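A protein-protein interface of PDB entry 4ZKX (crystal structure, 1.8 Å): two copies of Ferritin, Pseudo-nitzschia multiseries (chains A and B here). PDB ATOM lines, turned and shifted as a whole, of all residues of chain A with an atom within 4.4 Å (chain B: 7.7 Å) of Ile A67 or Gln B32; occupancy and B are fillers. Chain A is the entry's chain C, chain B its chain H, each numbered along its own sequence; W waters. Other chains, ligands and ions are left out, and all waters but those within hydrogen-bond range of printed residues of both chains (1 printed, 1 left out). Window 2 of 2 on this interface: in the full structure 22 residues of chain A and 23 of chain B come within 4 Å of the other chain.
The backbone carbonyl oxygen of Ile A67 sits at hydrogen-bond distance from NZ2 of YCM B78.
Printed residues of chain A that touch a printed residue of chain B: Asn A61, Ile A67, Glu A68 and Leu A69.
Along chain A the printed residues that touch a printed residue of chain B span positions 61 to 69.
Of the 16 printed residues of chain B, 6 touch a printed residue of chain A.
Among the printed residues, 11 pairs touch across the chains.
Water W1 lies within hydrogen-bond range of OD1 of Asn A61 (2.7 Å), O of Ile A65 (2.8 Å) and NE2 of Gln B32 (2.9 Å).
Ala A60 touches none of the printed residues of chain B.
Of the printed residues of chain B, Asn A61 touches Ile B28 (3.8 Å), Asp B31 (3.6 Å) and Gln B32 (3.98 Å).
Printed residues of chain B within 4 Å of Ile A67: Ile B28, Gln B32 and YCM B78.
Of the printed residues of chain A, Ser B25 touches Leu A69 (3.7 Å).
Of the printed residues of chain A, Asp B31 touches Asn A61.
Gln B32 touches two residues of chain A.
Ala B39 touches none of the printed residues of chain A.
No position is printed for both chains.
Of the 11 pairs that touch across the chains among the printed residues, none has its exchanged pair printed and touching as well.
OD1 of Asn A61 touches CG2 of Ile B28, at 3.8 Å.
Asp B31 touches Asn A61.
Gln B32 touches Asn A61 (CG to OD1, 3.98 Å).
Ile B28 touches Ile A67 (CD1 to CG2, 3.99 Å).
Ile A67 touches Gln B32.
NZ2 of YCM B78 touches CG of Glu A68 (3.8 Å).
Leu A69 touches Leu B24.
N of Ser B25 touches CD1 of Leu A69, at 3.7 Å.
Ile B28 touches Leu A69.
Leu A69 touches YCM B78 (N to OZ1, 3.7 Å).
The side-chain hydroxyl (OG) of Ser B25 lies close to OZ1 of YCM B78 (3.2 Å).
The side-chain amide oxygen of Asn A10 lies within hydrogen-bond range of the backbone NH of Glu A68 (2.8 Å).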
ATOM      1  N   ASN A  10      22.009 -24.208  -4.926  1.00  0.00           N
ATOM      2  CA  ASN A  10      21.486 -25.149  -5.923  1.00  0.00           C
ATOM      3  C   ASN A  10      19.918 -25.286  -5.865  1.00  0.00           C
ATOM      4  O   ASN A  10      19.212 -25.282  -6.913  1.00  0.00           O
ATOM      5  CB  ASN A  10      22.360 -26.457  -5.836  1.00  0.00           C
ATOM      6  CG  ASN A  10      22.122 -27.378  -6.952  1.00  0.00           C
ATOM      7  OD1 ASN A  10      22.549 -27.171  -8.054  1.00  0.00           O
ATOM      8  ND2 ASN A  10      21.297 -28.336  -6.702  1.00  0.00           N
ATOM      9  N   VAL A  13      17.973 -22.222  -7.493  1.00  0.00           N
ATOM     10  CA  VAL A  13      17.719 -22.359  -8.911  1.00  0.00           C
ATOM     11  C   VAL A  13      16.392 -23.103  -9.149  1.00  0.00           C
ATOM     12  O   VAL A  13      15.528 -22.677  -9.969  1.00  0.00           O
ATOM     13  CB  VAL A  13      18.884 -23.062  -9.652  1.00  0.00           C
ATOM     14  CG1 VAL A  13      18.486 -23.362 -11.077  1.00  0.00           C
ATOM     15  CG2 VAL A  13      20.176 -22.201  -9.610  1.00  0.00           C
ATOM     16  N   ALA A  60      26.585 -18.806 -10.084  1.00  0.00           N
ATOM     17  CA  ALA A  60      27.127 -20.047  -9.573  1.00  0.00           C
ATOM     18  C   ALA A  60      28.266 -20.530 -10.467  1.00  0.00           C
ATOM     19  O   ALA A  60      29.347 -20.918  -9.962  1.00  0.00           O
ATOM     20  CB  ALA A  60      26.044 -21.074  -9.508  1.00  0.00           C
ATOM     21  N   ASN A  61      28.044 -20.553 -11.781  1.00  0.00           N
ATOM     22  CA  ASN A  61      29.097 -20.957 -12.707  1.00  0.00           C
ATOM     23  C   ASN A  61      30.367 -20.084 -12.506  1.00  0.00           C
ATOM     24  O   ASN A  61      31.471 -20.601 -12.425  1.00  0.00           O
ATOM     25  CB  ASN A  61      28.654 -20.835 -14.158  1.00  0.00           C
ATOM     26  CG  ASN A  61      27.543 -21.864 -14.570  1.00  0.00           C
ATOM     27  OD1 ASN A  61      27.308 -22.863 -13.859  1.00  0.00           O
ATOM     28  ND2 ASN A  61      26.832 -21.573 -15.685  1.00  0.00           N
ATOM     29  N   ILE A  65      30.320 -22.578  -7.869  1.00  0.00           N
ATOM     30  CA  ILE A  65      29.312 -23.287  -7.058  1.00  0.00           C
ATOM     31  C   ILE A  65      28.735 -24.347  -7.993  1.00  0.00           C
ATOM     32  O   ILE A  65      28.116 -24.020  -8.995  1.00  0.00           O
ATOM     33  CB  ILE A  65      28.220 -22.324  -6.601  1.00  0.00           C
ATOM     34  CG1 ILE A  65      28.808 -21.256  -5.686  1.00  0.00           C
ATOM     35  CG2 ILE A  65      27.076 -23.039  -5.917  1.00  0.00           C
ATOM     36  CD1 ILE A  65      27.887 -20.050  -5.401  1.00  0.00           C
ATOM     37  N   PRO A  66      28.988 -25.653  -7.727  1.00  0.00           N
ATOM     38  CA  PRO A  66      28.427 -26.618  -8.707  1.00  0.00           C
ATOM     39  C   PRO A  66      26.919 -26.578  -8.766  1.00  0.00           C
ATOM     40  O   PRO A  66      26.200 -26.454  -7.747  1.00  0.00           O
ATOM     41  CB  PRO A  66      28.912 -28.004  -8.195  1.00  0.00           C
ATOM     42  CG  PRO A  66      29.737 -27.751  -6.959  1.00  0.00           C
ATOM     43  CD  PRO A  66      29.796 -26.277  -6.658  1.00  0.00           C
ATOM     44  N   ILE A  67      26.383 -26.668  -9.941  1.00  0.00           N
ATOM     45  CA  ILE A  67      24.942 -26.626 -10.104  1.00  0.00           C
ATOM     46  C   ILE A  67      24.661 -27.934 -10.722  1.00  0.00           C
ATOM     47  O   ILE A  67      25.398 -28.318 -11.636  1.00  0.00           O
ATOM     48  CB  ILE A  67      24.469 -25.524 -11.126  1.00  0.00           C
ATOM     49  CG1 ILE A  67      24.649 -24.162 -10.560  1.00  0.00           C
ATOM     50  CG2 ILE A  67      22.955 -25.733 -11.556  1.00  0.00           C
ATOM     51  CD1 ILE A  67      23.913 -23.947  -9.248  1.00  0.00           C
ATOM     52  N   GLU A  68      23.636 -28.609 -10.242  1.00  0.00           N
ATOM     53  CA  GLU A  68      23.084 -29.683 -11.020  1.00  0.00           C
ATOM     54  C   GLU A  68      21.564 -29.529 -11.069  1.00  0.00           C
ATOM     55  O   GLU A  68      20.893 -29.479 -10.013  1.00  0.00           O
ATOM     56  CB  GLU A  68      23.513 -31.039 -10.457  1.00  0.00           C
ATOM     57  CG  GLU A  68      24.980 -31.247 -10.826  1.00  0.00           C
ATOM     58  CD  GLU A  68      25.473 -32.669 -10.742  1.00  0.00           C
ATOM     59  OE1 GLU A  68      24.891 -33.407  -9.919  1.00  0.00           O
ATOM     60  OE2 GLU A  68      26.460 -32.990 -11.481  1.00  0.00           O
ATOM     61  N   LEU A  69      21.066 -29.452 -12.315  1.00  0.00           N
ATOM     62  CA  LEU A  69      19.669 -29.199 -12.492  1.00  0.00           C
ATOM     63  C   LEU A  69      18.838 -30.370 -11.941  1.00  0.00           C
ATOM     64  O   LEU A  69      19.073 -31.574 -12.245  1.00  0.00           O
ATOM     65  CB  LEU A  69      19.356 -28.947 -13.933  1.00  0.00           C
ATOM     66  CG  LEU A  69      20.004 -27.705 -14.558  1.00  0.00           C
ATOM     67  CD1 LEU A  69      19.656 -27.574 -16.007  1.00  0.00           C
ATOM     68  CD2 LEU A  69      19.478 -26.454 -13.756  1.00  0.00           C
ATOM     69  N   LEU B  24      19.779 -26.272 -21.294  1.00  0.00           N
ATOM     70  CA  LEU B  24      20.285 -25.559 -20.184  1.00  0.00           C
ATOM     71  C   LEU B  24      21.431 -26.348 -19.521  1.00  0.00           C
ATOM     72  O   LEU B  24      22.478 -25.794 -19.182  1.00  0.00           O
ATOM     73  CB  LEU B  24      19.188 -25.125 -19.243  1.00  0.00           C
ATOM     74  CG  LEU B  24      19.653 -24.354 -17.991  1.00  0.00           C
ATOM     75  CD1 LEU B  24      20.353 -23.078 -18.451  1.00  0.00           C
ATOM     76  CD2 LEU B  24      18.465 -24.051 -17.065  1.00  0.00           C
ATOM     77  N   SER B  25      21.208 -27.657 -19.330  1.00  0.00           N
ATOM     78  CA  SER B  25      22.236 -28.506 -18.783  1.00  0.00           C
ATOM     79  C   SER B  25      23.531 -28.408 -19.613  1.00  0.00           C
ATOM     80  O   SER B  25      24.622 -28.262 -19.025  1.00  0.00           O
ATOM     81  CB  SER B  25      21.746 -29.966 -18.647  1.00  0.00           C
ATOM     82  OG  SER B  25      22.745 -30.790 -18.076  1.00  0.00           O
ATOM     83  N   ALA B  26      23.403 -28.505 -20.945  1.00  0.00           N
ATOM     84  CA  ALA B  26      24.559 -28.408 -21.873  1.00  0.00           C
ATOM     85  C   ALA B  26      25.235 -27.052 -21.703  1.00  0.00           C
ATOM     86  O   ALA B  26      26.467 -26.993 -21.646  1.00  0.00           O
ATOM     87  CB  ALA B  26      24.118 -28.669 -23.282  1.00  0.00           C
ATOM     88  N   SER B  27      24.465 -25.974 -21.577  1.00  0.00           N
ATOM     89  CA  SER B  27      25.048 -24.658 -21.379  1.00  0.00           C
ATOM     90  C   SER B  27      25.884 -24.569 -20.106  1.00  0.00           C
ATOM     91  O   SER B  27      26.985 -24.046 -20.116  1.00  0.00           O
ATOM     92  CB  SER B  27      23.948 -23.612 -21.396  1.00  0.00           C
ATOM     93  OG  SER B  27      24.521 -22.300 -21.386  1.00  0.00           O
ATOM     94  N   ILE B  28      25.374 -25.161 -19.015  1.00  0.00           N
ATOM     95  CA  ILE B  28      26.089 -25.260 -17.767  1.00  0.00           C
ATOM     96  C   ILE B  28      27.378 -26.035 -17.904  1.00  0.00           C
ATOM     97  O   ILE B  28      28.410 -25.551 -17.472  1.00  0.00           O
ATOM     98  CB  ILE B  28      25.198 -25.791 -16.602  1.00  0.00           C
ATOM     99  CG1 ILE B  28      24.024 -24.852 -16.358  1.00  0.00           C
ATOM    100  CG2 ILE B  28      26.082 -26.118 -15.383  1.00  0.00           C
ATOM    101  CD1 ILE B  28      22.936 -25.486 -15.537  1.00  0.00           C
ATOM    102  N   TRP B  29      27.368 -27.202 -18.557  1.00  0.00           N
ATOM    103  CA  TRP B  29      28.574 -28.001 -18.701  1.00  0.00           C
ATOM    104  C   TRP B  29      29.606 -27.165 -19.476  1.00  0.00           C
ATOM    105  O   TRP B  29      30.775 -27.037 -19.091  1.00  0.00           O
ATOM    106  CB  TRP B  29      28.279 -29.338 -19.450  1.00  0.00           C
ATOM    107  CG  TRP B  29      29.445 -30.239 -19.445  1.00  0.00           C
ATOM    108  CD1 TRP B  29      29.717 -31.232 -18.537  1.00  0.00           C
ATOM    109  CD2 TRP B  29      30.544 -30.231 -20.364  1.00  0.00           C
ATOM    110  NE1 TRP B  29      30.927 -31.811 -18.803  1.00  0.00           N
ATOM    111  CE2 TRP B  29      31.469 -31.225 -19.912  1.00  0.00           C
ATOM    112  CE3 TRP B  29      30.897 -29.422 -21.437  1.00  0.00           C
ATOM    113  CZ2 TRP B  29      32.692 -31.465 -20.561  1.00  0.00           C
ATOM    114  CZ3 TRP B  29      32.106 -29.654 -22.099  1.00  0.00           C
ATOM    115  CH2 TRP B  29      32.990 -30.698 -21.663  1.00  0.00           C
ATOM    116  N   PHE B  30      29.141 -26.520 -20.525  1.00  0.00           N
ATOM    117  CA  PHE B  30      30.084 -25.750 -21.373  1.00  0.00           C
ATOM    118  C   PHE B  30      30.624 -24.579 -20.528  1.00  0.00           C
ATOM    119  O   PHE B  30      31.852 -24.338 -20.519  1.00  0.00           O
ATOM    120  CB  PHE B  30      29.431 -25.265 -22.678  1.00  0.00           C
ATOM    121  CG  PHE B  30      29.291 -26.299 -23.723  1.00  0.00           C
ATOM    122  CD1 PHE B  30      30.387 -27.119 -24.118  1.00  0.00           C
ATOM    123  CD2 PHE B  30      28.090 -26.450 -24.386  1.00  0.00           C
ATOM    124  CE1 PHE B  30      30.227 -28.035 -25.141  1.00  0.00           C
ATOM    125  CE2 PHE B  30      27.943 -27.355 -25.397  1.00  0.00           C
ATOM    126  CZ  PHE B  30      29.019 -28.172 -25.764  1.00  0.00           C
ATOM    127  N   ASP B  31      29.755 -23.837 -19.810  1.00  0.00           N
ATOM    128  CA  ASP B  31      30.313 -22.689 -18.988  1.00  0.00           C
ATOM    129  C   ASP B  31      31.285 -23.143 -17.939  1.00  0.00           C
ATOM    130  O   ASP B  31      32.350 -22.515 -17.732  1.00  0.00           O
ATOM    131  CB  ASP B  31      29.223 -21.829 -18.334  1.00  0.00           C
ATOM    132  CG  ASP B  31      28.713 -20.722 -19.258  1.00  0.00           C
ATOM    133  OD1 ASP B  31      29.582 -20.081 -19.939  1.00  0.00           O
ATOM    134  OD2 ASP B  31      27.438 -20.516 -19.335  1.00  0.00           O
ATOM    135  N   GLN B  32      30.963 -24.264 -17.271  1.00  0.00           N
ATOM    136  CA  GLN B  32      31.827 -24.756 -16.189  1.00  0.00           C
ATOM    137  C   GLN B  32      33.156 -25.160 -16.728  1.00  0.00           C
ATOM    138  O   GLN B  32      34.128 -25.125 -15.975  1.00  0.00           O
ATOM    139  CB  GLN B  32      31.209 -25.970 -15.475  1.00  0.00           C
ATOM    140  CG  GLN B  32      30.012 -25.673 -14.642  1.00  0.00           C
ATOM    141  CD  GLN B  32      29.322 -26.959 -14.113  1.00  0.00           C
ATOM    142  OE1 GLN B  32      29.346 -28.044 -14.755  1.00  0.00           O
ATOM    143  NE2 GLN B  32      28.631 -26.807 -13.003  1.00  0.00           N
ATOM    144  N   ASN B  33      33.221 -25.595 -17.992  1.00  0.00           N
ATOM    145  CA  ASN B  33      34.458 -26.022 -18.622  1.00  0.00           C
ATOM    146  C   ASN B  33      35.079 -24.961 -19.574  1.00  0.00           C
ATOM    147  O   ASN B  33      35.904 -25.272 -20.395  1.00  0.00           O
ATOM    148  CB  ASN B  33      34.255 -27.395 -19.316  1.00  0.00           C
ATOM    149  CG  ASN B  33      34.049 -28.490 -18.277  1.00  0.00           C
ATOM    150  OD1 ASN B  33      35.010 -28.942 -17.689  1.00  0.00           O
ATOM    151  ND2 ASN B  33      32.810 -28.845 -17.976  1.00  0.00           N
ATOM    152  N   ASP B  34      34.603 -23.738 -19.431  1.00  0.00           N
ATOM    153  CA  ASP B  34      35.073 -22.517 -20.164  1.00  0.00           C
ATOM    154  C   ASP B  34      34.928 -22.598 -21.694  1.00  0.00           C
ATOM    155  O   ASP B  34      35.833 -22.180 -22.432  1.00  0.00           O
ATOM    156  CB  ASP B  34      36.516 -22.219 -19.735  1.00  0.00           C
ATOM    157  CG  ASP B  34      36.641 -22.135 -18.215  1.00  0.00           C
ATOM    158  OD1 ASP B  34      35.950 -21.300 -17.580  1.00  0.00           O
ATOM    159  OD2 ASP B  34      37.345 -22.987 -17.701  1.00  0.00           O
ATOM    160  N   TRP B  35      33.797 -23.143 -22.179  1.00  0.00           N
ATOM    161  CA  TRP B  35      33.441 -23.109 -23.579  1.00  0.00           C
ATOM    162  C   TRP B  35      32.285 -22.074 -23.649  1.00  0.00           C
ATOM    163  O   TRP B  35      31.157 -22.432 -23.916  1.00  0.00           O
ATOM    164  CB  TRP B  35      33.002 -24.484 -24.080  1.00  0.00           C
ATOM    165  CG  TRP B  35      34.037 -25.535 -24.017  1.00  0.00           C
ATOM    166  CD1 TRP B  35      34.275 -26.393 -22.991  1.00  0.00           C
ATOM    167  CD2 TRP B  35      34.980 -25.839 -25.025  1.00  0.00           C
ATOM    168  NE1 TRP B  35      35.355 -27.220 -23.295  1.00  0.00           N
ATOM    169  CE2 TRP B  35      35.791 -26.898 -24.546  1.00  0.00           C
ATOM    170  CE3 TRP B  35      35.191 -25.342 -26.314  1.00  0.00           C
ATOM    171  CZ2 TRP B  35      36.852 -27.423 -25.295  1.00  0.00           C
ATOM    172  CZ3 TRP B  35      36.184 -25.880 -27.067  1.00  0.00           C
ATOM    173  CH2 TRP B  35      36.999 -26.911 -26.557  1.00  0.00           C
ATOM    174  N   GLU B  36      32.551 -20.768 -23.434  1.00  0.00           N
ATOM    175  CA  GLU B  36      31.496 -19.786 -23.285  1.00  0.00           C
ATOM    176  C   GLU B  36      30.704 -19.601 -24.631  1.00  0.00           C
ATOM    177  O   GLU B  36      29.500 -19.310 -24.612  1.00  0.00           O
ATOM    178  CB  GLU B  36      32.016 -18.430 -22.761  1.00  0.00           C
ATOM    179  CG  GLU B  36      32.489 -18.425 -21.322  1.00  0.00           C
ATOM    180  CD  GLU B  36      33.969 -18.862 -21.200  1.00  0.00           C
ATOM    181  OE1 GLU B  36      34.601 -19.117 -22.243  1.00  0.00           O
ATOM    182  OE2 GLU B  36      34.461 -18.926 -20.042  1.00  0.00           O
ATOM    183  N   ALA B  39      28.339 -22.474 -24.842  1.00  0.00           N
ATOM    184  CA  ALA B  39      27.394 -22.292 -23.772  1.00  0.00           C
ATOM    185  C   ALA B  39      26.332 -21.338 -24.135  1.00  0.00           C
ATOM    186  O   ALA B  39      25.188 -21.507 -23.817  1.00  0.00           O
ATOM    187  CB  ALA B  39      28.126 -21.780 -22.550  1.00  0.00           C
ATOM    188  N   YCM B  78      24.490 -34.991 -18.581  1.00  0.00           N
ATOM    189  CA  YCM B  78      25.604 -34.187 -17.976  1.00  0.00           C
ATOM    190  CB  YCM B  78      25.054 -32.905 -17.294  1.00  0.00           C
ATOM    191  SG  YCM B  78      26.325 -31.803 -16.562  1.00  0.00           S
ATOM    192  CD  YCM B  78      25.404 -30.132 -16.574  1.00  0.00           C
ATOM    193  CE  YCM B  78      24.768 -29.791 -15.262  1.00  0.00           C
ATOM    194  OZ1 YCM B  78      23.505 -29.750 -15.119  1.00  0.00           O
ATOM    195  NZ2 YCM B  78      25.654 -29.589 -14.222  1.00  0.00           N
ATOM    196  C   YCM B  78      26.479 -34.986 -17.025  1.00  0.00           C
ATOM    197  O   YCM B  78      27.748 -34.772 -16.971  1.00  0.00           O
ATOM    198  N   ARG B 153      39.132 -25.468 -29.265  1.00  0.00           N
ATOM    199  CA  ARG B 153      39.085 -24.192 -28.493  1.00  0.00           C
ATOM    200  C   ARG B 153      39.074 -22.966 -29.389  1.00  0.00           C
ATOM    201  O   ARG B 153      38.286 -22.033 -29.153  1.00  0.00           O
ATOM    202  CB  ARG B 153      40.230 -24.274 -27.442  1.00  0.00           C
ATOM    203  CG  ARG B 153      40.077 -23.636 -26.116  1.00  0.00           C
ATOM    204  CD  ARG B 153      38.927 -24.022 -25.280  1.00  0.00           C
ATOM    205  NE  ARG B 153      39.318 -25.024 -24.312  1.00  0.00           N
ATOM    206  CZ  ARG B 153      38.648 -25.278 -23.197  1.00  0.00           C
ATOM    207  NH1 ARG B 153      37.662 -24.525 -22.831  1.00  0.00           N
ATOM    208  NH2 ARG B 153      39.039 -26.245 -22.412  1.00  0.00           N
HETATM  209  O   HOH W   1      28.359 -24.233 -11.800  1.00  0.00           O
